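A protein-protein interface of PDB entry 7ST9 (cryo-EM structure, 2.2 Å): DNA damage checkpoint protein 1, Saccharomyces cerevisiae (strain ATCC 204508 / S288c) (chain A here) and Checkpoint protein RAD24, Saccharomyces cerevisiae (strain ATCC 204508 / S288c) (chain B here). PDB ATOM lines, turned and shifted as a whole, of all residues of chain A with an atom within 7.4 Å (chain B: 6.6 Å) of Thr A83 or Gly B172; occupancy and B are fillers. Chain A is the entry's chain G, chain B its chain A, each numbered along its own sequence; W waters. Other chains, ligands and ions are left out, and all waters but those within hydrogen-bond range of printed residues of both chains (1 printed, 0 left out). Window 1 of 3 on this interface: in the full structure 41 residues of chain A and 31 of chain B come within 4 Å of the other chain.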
ATOM      1  N   MET A  78     -16.484  -7.647 -29.991  1.00  0.00           N
ATOM      2  CA  MET A  78     -16.141  -7.826 -28.587  1.00  0.00           C
ATOM      3  C   MET A  78     -15.961  -9.312 -28.319  1.00  0.00           C
ATOM      4  O   MET A  78     -16.734 -10.136 -28.814  1.00  0.00           O
ATOM      5  CB  MET A  78     -17.226  -7.249 -27.667  1.00  0.00           C
ATOM      6  CG  MET A  78     -16.685  -6.466 -26.480  1.00  0.00           C
ATOM      7  SD  MET A  78     -17.885  -6.274 -25.147  1.00  0.00           S
ATOM      8  CE  MET A  78     -19.146  -5.294 -25.960  1.00  0.00           C
ATOM      9  N   ASN A  79     -14.941  -9.653 -27.537  1.00  0.00           N
ATOM     10  CA  ASN A  79     -14.645 -11.053 -27.278  1.00  0.00           C
ATOM     11  C   ASN A  79     -15.594 -11.616 -26.220  1.00  0.00           C
ATOM     12  O   ASN A  79     -16.367 -10.896 -25.584  1.00  0.00           O
ATOM     13  CB  ASN A  79     -13.188 -11.225 -26.850  1.00  0.00           C
ATOM     14  CG  ASN A  79     -12.926 -10.738 -25.440  1.00  0.00           C
ATOM     15  OD1 ASN A  79     -13.664  -9.912 -24.904  1.00  0.00           O
ATOM     16  ND2 ASN A  79     -11.859 -11.243 -24.834  1.00  0.00           N
ATOM     17  N   GLU A  80     -15.525 -12.938 -26.041  1.00  0.00           N
ATOM     18  CA  GLU A  80     -16.474 -13.619 -25.165  1.00  0.00           C
ATOM     19  C   GLU A  80     -16.348 -13.138 -23.723  1.00  0.00           C
ATOM     20  O   GLU A  80     -17.357 -12.983 -23.026  1.00  0.00           O
ATOM     21  CB  GLU A  80     -16.262 -15.131 -25.248  1.00  0.00           C
ATOM     22  CG  GLU A  80     -17.460 -15.966 -24.804  1.00  0.00           C
ATOM     23  CD  GLU A  80     -18.729 -15.640 -25.572  1.00  0.00           C
ATOM     24  OE1 GLU A  80     -18.955 -16.249 -26.638  1.00  0.00           O
ATOM     25  OE2 GLU A  80     -19.498 -14.774 -25.107  1.00  0.00           O
ATOM     26  N   THR A  81     -15.124 -12.900 -23.257  1.00  0.00           N
ATOM     27  CA  THR A  81     -14.897 -12.477 -21.880  1.00  0.00           C
ATOM     28  C   THR A  81     -15.184 -10.999 -21.655  1.00  0.00           C
ATOM     29  O   THR A  81     -15.101 -10.540 -20.511  1.00  0.00           O
ATOM     30  CB  THR A  81     -13.453 -12.778 -21.463  1.00  0.00           C
ATOM     31  OG1 THR A  81     -12.546 -12.197 -22.408  1.00  0.00           O
ATOM     32  CG2 THR A  81     -13.218 -14.279 -21.388  1.00  0.00           C
ATOM     33  N   ASP A  82     -15.504 -10.245 -22.706  1.00  0.00           N
ATOM     34  CA  ASP A  82     -15.792  -8.816 -22.595  1.00  0.00           C
ATOM     35  C   ASP A  82     -14.590  -8.037 -22.066  1.00  0.00           C
ATOM     36  O   ASP A  82     -14.742  -6.994 -21.427  1.00  0.00           O
ATOM     37  CB  ASP A  82     -17.021  -8.565 -21.713  1.00  0.00           C
ATOM     38  CG  ASP A  82     -18.324  -8.716 -22.470  1.00  0.00           C
ATOM     39  OD1 ASP A  82     -18.539  -9.781 -23.085  1.00  0.00           O
ATOM     40  OD2 ASP A  82     -19.135  -7.767 -22.449  1.00  0.00           O
ATOM     41  N   THR A  83     -13.382  -8.537 -22.327  1.00  0.00           N
ATOM     42  CA  THR A  83     -12.161  -7.864 -21.907  1.00  0.00           C
ATOM     43  C   THR A  83     -11.543  -7.002 -23.000  1.00  0.00           C
ATOM     44  O   THR A  83     -10.601  -6.256 -22.715  1.00  0.00           O
ATOM     45  CB  THR A  83     -11.124  -8.894 -21.435  1.00  0.00           C
ATOM     46  OG1 THR A  83     -10.995  -9.932 -22.414  1.00  0.00           O
ATOM     47  CG2 THR A  83     -11.537  -9.501 -20.103  1.00  0.00           C
ATOM     48  N   THR A  84     -12.044  -7.081 -24.231  1.00  0.00           N
ATOM     49  CA  THR A  84     -11.498  -6.313 -25.341  1.00  0.00           C
ATOM     50  C   THR A  84     -12.615  -5.933 -26.303  1.00  0.00           C
ATOM     51  O   THR A  84     -13.487  -6.750 -26.610  1.00  0.00           O
ATOM     52  CB  THR A  84     -10.420  -7.101 -26.094  1.00  0.00           C
ATOM     53  OG1 THR A  84     -10.020  -6.375 -27.263  1.00  0.00           O
ATOM     54  CG2 THR A  84     -10.948  -8.466 -26.507  1.00  0.00           C
ATOM     55  N   LEU A  85     -12.573  -4.691 -26.778  1.00  0.00           N
ATOM     56  CA  LEU A  85     -13.528  -4.179 -27.751  1.00  0.00           C
ATOM     57  C   LEU A  85     -12.760  -3.468 -28.854  1.00  0.00           C
ATOM     58  O   LEU A  85     -11.896  -2.634 -28.568  1.00  0.00           O
ATOM     59  CB  LEU A  85     -14.529  -3.223 -27.085  1.00  0.00           C
ATOM     60  CG  LEU A  85     -15.557  -2.484 -27.954  1.00  0.00           C
ATOM     61  CD1 LEU A  85     -14.953  -1.258 -28.631  1.00  0.00           C
ATOM     62  CD2 LEU A  85     -16.181  -3.411 -28.987  1.00  0.00           C
ATOM     63  N   PHE A 358      -1.644  -5.503 -19.605  1.00  0.00           N
ATOM     64  CA  PHE A 358      -2.829  -6.014 -20.289  1.00  0.00           C
ATOM     65  C   PHE A 358      -2.402  -7.108 -21.263  1.00  0.00           C
ATOM     66  O   PHE A 358      -1.249  -7.551 -21.262  1.00  0.00           O
ATOM     67  CB  PHE A 358      -3.597  -4.881 -20.984  1.00  0.00           C
ATOM     68  CG  PHE A 358      -2.739  -3.991 -21.836  1.00  0.00           C
ATOM     69  CD1 PHE A 358      -2.024  -2.949 -21.271  1.00  0.00           C
ATOM     70  CD2 PHE A 358      -2.657  -4.185 -23.205  1.00  0.00           C
ATOM     71  CE1 PHE A 358      -1.238  -2.126 -22.050  1.00  0.00           C
ATOM     72  CE2 PHE A 358      -1.874  -3.361 -23.991  1.00  0.00           C
ATOM     73  CZ  PHE A 358      -1.163  -2.333 -23.412  1.00  0.00           C
ATOM     74  N   LYS A 359      -3.349  -7.570 -22.075  1.00  0.00           N
ATOM     75  CA  LYS A 359      -3.085  -8.621 -23.045  1.00  0.00           C
ATOM     76  C   LYS A 359      -2.428  -8.044 -24.294  1.00  0.00           C
ATOM     77  O   LYS A 359      -2.712  -6.916 -24.708  1.00  0.00           O
ATOM     78  CB  LYS A 359      -4.382  -9.340 -23.418  1.00  0.00           C
ATOM     79  CG  LYS A 359      -4.309 -10.851 -23.296  1.00  0.00           C
ATOM     80  CD  LYS A 359      -5.653 -11.496 -23.590  1.00  0.00           C
ATOM     81  CE  LYS A 359      -5.506 -12.981 -23.863  1.00  0.00           C
ATOM     82  NZ  LYS A 359      -4.996 -13.250 -25.234  1.00  0.00           N
ATOM     83  N   ASP A 362      -4.292  -8.798 -28.811  1.00  0.00           N
ATOM     84  CA  ASP A 362      -5.221  -7.871 -29.446  1.00  0.00           C
ATOM     85  C   ASP A 362      -4.519  -6.591 -29.875  1.00  0.00           C
ATOM     86  O   ASP A 362      -4.770  -6.080 -30.969  1.00  0.00           O
ATOM     87  CB  ASP A 362      -6.376  -7.559 -28.497  1.00  0.00           C
ATOM     88  CG  ASP A 362      -7.556  -8.487 -28.693  1.00  0.00           C
ATOM     89  OD1 ASP A 362      -7.437  -9.458 -29.470  1.00  0.00           O
ATOM     90  OD2 ASP A 362      -8.606  -8.246 -28.069  1.00  0.00           O
ATOM     91  N   ILE A 394      -7.983   0.590 -20.729  1.00  0.00           N
ATOM     92  CA  ILE A 394      -6.991   1.325 -21.503  1.00  0.00           C
ATOM     93  C   ILE A 394      -7.547   1.517 -22.907  1.00  0.00           C
ATOM     94  O   ILE A 394      -7.988   0.550 -23.546  1.00  0.00           O
ATOM     95  CB  ILE A 394      -5.633   0.602 -21.538  1.00  0.00           C
ATOM     96  CG1 ILE A 394      -4.631   1.402 -22.375  1.00  0.00           C
ATOM     97  CG2 ILE A 394      -5.772  -0.807 -22.100  1.00  0.00           C
ATOM     98  CD1 ILE A 394      -3.188   1.015 -22.139  1.00  0.00           C
ATOM     99  N   VAL A 408     -10.249  -0.914 -26.944  1.00  0.00           N
ATOM    100  CA  VAL A 408     -10.372  -0.776 -25.498  1.00  0.00           C
ATOM    101  C   VAL A 408     -10.066  -2.127 -24.871  1.00  0.00           C
ATOM    102  O   VAL A 408     -10.614  -3.149 -25.296  1.00  0.00           O
ATOM    103  CB  VAL A 408     -11.775  -0.289 -25.088  1.00  0.00           C
ATOM    104  CG1 VAL A 408     -11.842  -0.069 -23.583  1.00  0.00           C
ATOM    105  CG2 VAL A 408     -12.136   0.984 -25.836  1.00  0.00           C
ATOM    106  N   GLU A 409      -9.189  -2.131 -23.868  1.00  0.00           N
ATOM    107  CA  GLU A 409      -8.782  -3.365 -23.209  1.00  0.00           C
ATOM    108  C   GLU A 409      -8.905  -3.215 -21.699  1.00  0.00           C
ATOM    109  O   GLU A 409      -8.858  -2.111 -21.156  1.00  0.00           O
ATOM    110  CB  GLU A 409      -7.344  -3.754 -23.581  1.00  0.00           C
ATOM    111  CG  GLU A 409      -7.250  -4.710 -24.763  1.00  0.00           C
ATOM    112  CD  GLU A 409      -5.900  -5.392 -24.864  1.00  0.00           C
ATOM    113  OE1 GLU A 409      -5.296  -5.684 -23.810  1.00  0.00           O
ATOM    114  OE2 GLU A 409      -5.442  -5.640 -25.998  1.00  0.00           O
ATOM    115  N   VAL A 410      -9.067  -4.349 -21.021  1.00  0.00           N
ATOM    116  CA  VAL A 410      -9.149  -4.384 -19.565  1.00  0.00           C
ATOM    117  C   VAL A 410      -7.750  -4.605 -19.006  1.00  0.00           C
ATOM    118  O   VAL A 410      -7.044  -5.533 -19.419  1.00  0.00           O
ATOM    119  CB  VAL A 410     -10.114  -5.486 -19.094  1.00  0.00           C
ATOM    120  CG1 VAL A 410      -9.960  -5.731 -17.598  1.00  0.00           C
ATOM    121  CG2 VAL A 410     -11.551  -5.114 -19.430  1.00  0.00           C
ATOM    122  N   THR A 411      -7.351  -3.757 -18.065  1.00  0.00           N
ATOM    123  CA  THR A 411      -6.014  -3.785 -17.492  1.00  0.00           C
ATOM    124  C   THR A 411      -5.998  -4.558 -16.176  1.00  0.00           C
ATOM    125  O   THR A 411      -7.027  -4.755 -15.527  1.00  0.00           O
ATOM    126  CB  THR A 411      -5.494  -2.363 -17.262  1.00  0.00           C
ATOM    127  OG1 THR A 411      -6.357  -1.677 -16.346  1.00  0.00           O
ATOM    128  CG2 THR A 411      -5.437  -1.593 -18.574  1.00  0.00           C
ATOM    129  N   PHE B 139     -17.607   0.166 -19.722  1.00  0.00           N
ATOM    130  CA  PHE B 139     -17.665   0.078 -21.177  1.00  0.00           C
ATOM    131  C   PHE B 139     -18.770   0.970 -21.731  1.00  0.00           C
ATOM    132  O   PHE B 139     -18.507   1.927 -22.468  1.00  0.00           O
ATOM    133  CB  PHE B 139     -17.878  -1.376 -21.602  1.00  0.00           C
ATOM    134  CG  PHE B 139     -16.601  -2.146 -21.793  1.00  0.00           C
ATOM    135  CD1 PHE B 139     -15.538  -1.980 -20.921  1.00  0.00           C
ATOM    136  CD2 PHE B 139     -16.467  -3.041 -22.842  1.00  0.00           C
ATOM    137  CE1 PHE B 139     -14.364  -2.688 -21.094  1.00  0.00           C
ATOM    138  CE2 PHE B 139     -15.295  -3.753 -23.018  1.00  0.00           C
ATOM    139  CZ  PHE B 139     -14.243  -3.575 -22.144  1.00  0.00           C
ATOM    140  N   SER B 167      -7.520 -21.991 -23.864  1.00  0.00           N
ATOM    141  CA  SER B 167      -6.376 -21.288 -23.296  1.00  0.00           C
ATOM    142  C   SER B 167      -6.567 -19.782 -23.396  1.00  0.00           C
ATOM    143  O   SER B 167      -6.258 -19.044 -22.454  1.00  0.00           O
ATOM    144  CB  SER B 167      -5.090 -21.714 -24.004  1.00  0.00           C
ATOM    145  OG  SER B 167      -4.014 -20.859 -23.664  1.00  0.00           O
ATOM    146  N   GLU B 168      -7.087 -19.307 -24.530  1.00  0.00           N
ATOM    147  CA  GLU B 168      -7.346 -17.880 -24.670  1.00  0.00           C
ATOM    148  C   GLU B 168      -8.392 -17.420 -23.663  1.00  0.00           C
ATOM    149  O   GLU B 168      -8.206 -16.410 -22.973  1.00  0.00           O
ATOM    150  CB  GLU B 168      -7.793 -17.568 -26.098  1.00  0.00           C
ATOM    151  CG  GLU B 168      -7.402 -16.182 -26.580  1.00  0.00           C
ATOM    152  CD  GLU B 168      -5.905 -16.028 -26.770  1.00  0.00           C
ATOM    153  OE1 GLU B 168      -5.209 -17.060 -26.886  1.00  0.00           O
ATOM    154  OE2 GLU B 168      -5.424 -14.877 -26.803  1.00  0.00           O
ATOM    155  N   PHE B 169      -9.484 -18.178 -23.534  1.00  0.00           N
ATOM    156  CA  PHE B 169     -10.578 -17.756 -22.666  1.00  0.00           C
ATOM    157  C   PHE B 169     -10.077 -17.488 -21.253  1.00  0.00           C
ATOM    158  O   PHE B 169     -10.296 -16.405 -20.696  1.00  0.00           O
ATOM    159  CB  PHE B 169     -11.677 -18.820 -22.659  1.00  0.00           C
ATOM    160  CG  PHE B 169     -12.801 -18.525 -21.707  1.00  0.00           C
ATOM    161  CD1 PHE B 169     -13.752 -17.567 -22.012  1.00  0.00           C
ATOM    162  CD2 PHE B 169     -12.905 -19.209 -20.506  1.00  0.00           C
ATOM    163  CE1 PHE B 169     -14.788 -17.294 -21.137  1.00  0.00           C
ATOM    164  CE2 PHE B 169     -13.938 -18.939 -19.627  1.00  0.00           C
ATOM    165  CZ  PHE B 169     -14.880 -17.982 -19.944  1.00  0.00           C
ATOM    166  N   LEU B 170      -9.367 -18.455 -20.669  1.00  0.00           N
ATOM    167  CA  LEU B 170      -8.837 -18.261 -19.325  1.00  0.00           C
ATOM    168  C   LEU B 170      -7.922 -17.048 -19.275  1.00  0.00           C
ATOM    169  O   LEU B 170      -7.997 -16.242 -18.338  1.00  0.00           O
ATOM    170  CB  LEU B 170      -8.095 -19.516 -18.865  1.00  0.00           C
ATOM    171  CG  LEU B 170      -8.952 -20.764 -18.635  1.00  0.00           C
ATOM    172  CD1 LEU B 170      -8.093 -21.922 -18.150  1.00  0.00           C
ATOM    173  CD2 LEU B 170     -10.081 -20.487 -17.651  1.00  0.00           C
ATOM    174  N   LYS B 171      -7.071 -16.878 -20.290  1.00  0.00           N
ATOM    175  CA  LYS B 171      -6.157 -15.744 -20.290  1.00  0.00           C
ATOM    176  C   LYS B 171      -6.901 -14.418 -20.249  1.00  0.00           C
ATOM    177  O   LYS B 171      -6.333 -13.413 -19.811  1.00  0.00           O
ATOM    178  CB  LYS B 171      -5.242 -15.802 -21.514  1.00  0.00           C
ATOM    179  CG  LYS B 171      -4.077 -16.762 -21.354  1.00  0.00           C
ATOM    180  CD  LYS B 171      -3.263 -16.877 -22.631  1.00  0.00           C
ATOM    181  CE  LYS B 171      -1.966 -17.633 -22.395  1.00  0.00           C
ATOM    182  NZ  LYS B 171      -2.204 -19.021 -21.906  1.00  0.00           N
ATOM    183  N   GLY B 172      -8.158 -14.392 -20.687  1.00  0.00           N
ATOM    184  CA  GLY B 172      -8.978 -13.210 -20.522  1.00  0.00           C
ATOM    185  C   GLY B 172      -9.686 -13.217 -19.183  1.00  0.00           C
ATOM    186  O   GLY B 172      -9.735 -12.199 -18.484  1.00  0.00           O
ATOM    187  N   ALA B 173     -10.217 -14.384 -18.805  1.00  0.00           N
ATOM    188  CA  ALA B 173     -11.010 -14.476 -17.584  1.00  0.00           C
ATOM    189  C   ALA B 173     -10.207 -14.058 -16.361  1.00  0.00           C
ATOM    190  O   ALA B 173     -10.783 -13.595 -15.370  1.00  0.00           O
ATOM    191  CB  ALA B 173     -11.538 -15.899 -17.412  1.00  0.00           C
ATOM    192  N   ARG B 174      -8.882 -14.207 -16.412  1.00  0.00           N
ATOM    193  CA  ARG B 174      -8.047 -13.814 -15.282  1.00  0.00           C
ATOM    194  C   ARG B 174      -8.266 -12.357 -14.899  1.00  0.00           C
ATOM    195  O   ARG B 174      -8.135 -12.001 -13.722  1.00  0.00           O
ATOM    196  CB  ARG B 174      -6.573 -14.053 -15.617  1.00  0.00           C
ATOM    197  CG  ARG B 174      -5.619 -13.803 -14.459  1.00  0.00           C
ATOM    198  CD  ARG B 174      -5.040 -12.393 -14.494  1.00  0.00           C
ATOM    199  NE  ARG B 174      -3.888 -12.285 -15.379  1.00  0.00           N
ATOM    200  CZ  ARG B 174      -3.069 -11.243 -15.418  1.00  0.00           C
ATOM    201  NH1 ARG B 174      -3.247 -10.194 -14.631  1.00  0.00           N
ATOM    202  NH2 ARG B 174      -2.047 -11.251 -16.268  1.00  0.00           N
ATOM    203  N   TYR B 175      -8.600 -11.501 -15.866  1.00  0.00           N
ATOM    204  CA  TYR B 175      -8.685 -10.070 -15.605  1.00  0.00           C
ATOM    205  C   TYR B 175      -9.990  -9.650 -14.942  1.00  0.00           C
ATOM    206  O   TYR B 175     -10.089  -8.505 -14.486  1.00  0.00           O
ATOM    207  CB  TYR B 175      -8.510  -9.291 -16.912  1.00  0.00           C
ATOM    208  CG  TYR B 175      -7.086  -9.256 -17.419  1.00  0.00           C
ATOM    209  CD1 TYR B 175      -6.604 -10.250 -18.260  1.00  0.00           C
ATOM    210  CD2 TYR B 175      -6.225  -8.230 -17.057  1.00  0.00           C
ATOM    211  CE1 TYR B 175      -5.303 -10.224 -18.726  1.00  0.00           C
ATOM    212  CE2 TYR B 175      -4.922  -8.194 -17.519  1.00  0.00           C
ATOM    213  CZ  TYR B 175      -4.467  -9.193 -18.352  1.00  0.00           C
ATOM    214  OH  TYR B 175      -3.171  -9.163 -18.814  1.00  0.00           O
ATOM    215  N   LEU B 176     -10.986 -10.535 -14.866  1.00  0.00           N
ATOM    216  CA  LEU B 176     -12.309 -10.175 -14.353  1.00  0.00           C
ATOM    217  C   LEU B 176     -12.315 -10.277 -12.826  1.00  0.00           C
ATOM    218  O   LEU B 176     -12.925 -11.163 -12.224  1.00  0.00           O
ATOM    219  CB  LEU B 176     -13.377 -11.062 -14.977  1.00  0.00           C
ATOM    220  CG  LEU B 176     -13.398 -11.093 -16.507  1.00  0.00           C
ATOM    221  CD1 LEU B 176     -14.350 -12.167 -17.010  1.00  0.00           C
ATOM    222  CD2 LEU B 176     -13.776  -9.730 -17.066  1.00  0.00           C
HETATM  223  O   HOH W   1      -8.477  -6.841 -13.757  1.00  0.00           O
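The side-chain carboxylate of Glu B168 sits close to the side-chain amino group of Lys A359, 2.3 Å away.
The side-chain hydroxyl (OG) of Ser B167 lies within hydrogen-bond range of the side-chain amino group (NZ) of Lys B171 (3.1 Å).
The side-chain hydroxyl of Tyr B175 sits at hydrogen-bond distance from the guanidinium group of Arg B174 (3.5 Å).
The backbone NH of Asp A82 sits at hydrogen-bond distance from the side-chain amide oxygen of Asn A79.
The side-chain amide nitrogen (ND2) of Asn A79 is in hydrogen-bond range of the side-chain hydroxyl (OG1) of Thr A83 (2.9 Å).
The side-chain hydroxyl (OG1) of Thr A83 lies within hydrogen-bond range of the side-chain hydroxyl (OG1) of Thr A81 (2.7 Å).
The backbone NH of Val A410 is in hydrogen-bond range of the backbone carbonyl oxygen of Thr A83 (3.0 Å).
Among the printed residues, merely in contact across the chains: Thr A81 with Phe B169, Thr A81 with Ala B173, Thr A81 with Leu B176, Asp A82 with Phe B139, Thr A83 with Gly B172, Thr A83 with Leu B176, Phe A358 with Tyr B175, Lys A359 with Lys B171, Lys A359 with Tyr B175, Val A410 with Tyr B175 and Thr A411 with Tyr B175.
Of the printed residues of chain A, Gly B172 touches Thr A83.
Of the printed residues of chain B, Thr A411 touches Tyr B175.
Of the printed residues of chain A, Phe B169 touches Thr A81 (3.4 Å).
Of the printed residues of chain A, Phe B139 touches Asp A82.
The nearest residue of chain B that does not touch Thr A83 is Tyr B175 (4.4 Å).
The nearest printed residue of chain B that does not touch Thr A411 is Arg B174 (6.5 Å).
Printed residues of chain B that touch a printed residue of chain A: Phe B139, Glu B168, Phe B169, Lys B171, Gly B172, Ala B173, Tyr B175 and Leu B176.
Hydrophobic or aromatic side chains of chain B within 4 Å of the printed part of chain A: Phe B139, Phe B169, Tyr B175 and Leu B176.
Printed residues of chain A that touch a printed residue of chain B: Thr A81, Asp A82, Thr A83, Phe A358, Lys A359, Val A410 and Thr A411.
Hydrophobic or aromatic side chains of chain A within 4 Å of the printed part of chain B: Val A410.
Among the printed residues, Asp or Glu carboxylates within 4 Å of a Lys or Arg side-chain nitrogen of the other chain: Lys A359 with Glu B168 (2.3 Å).
Water W1 bridges O of Tyr B175 (2.4 Å) and O of Thr A411 (3.1 Å).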
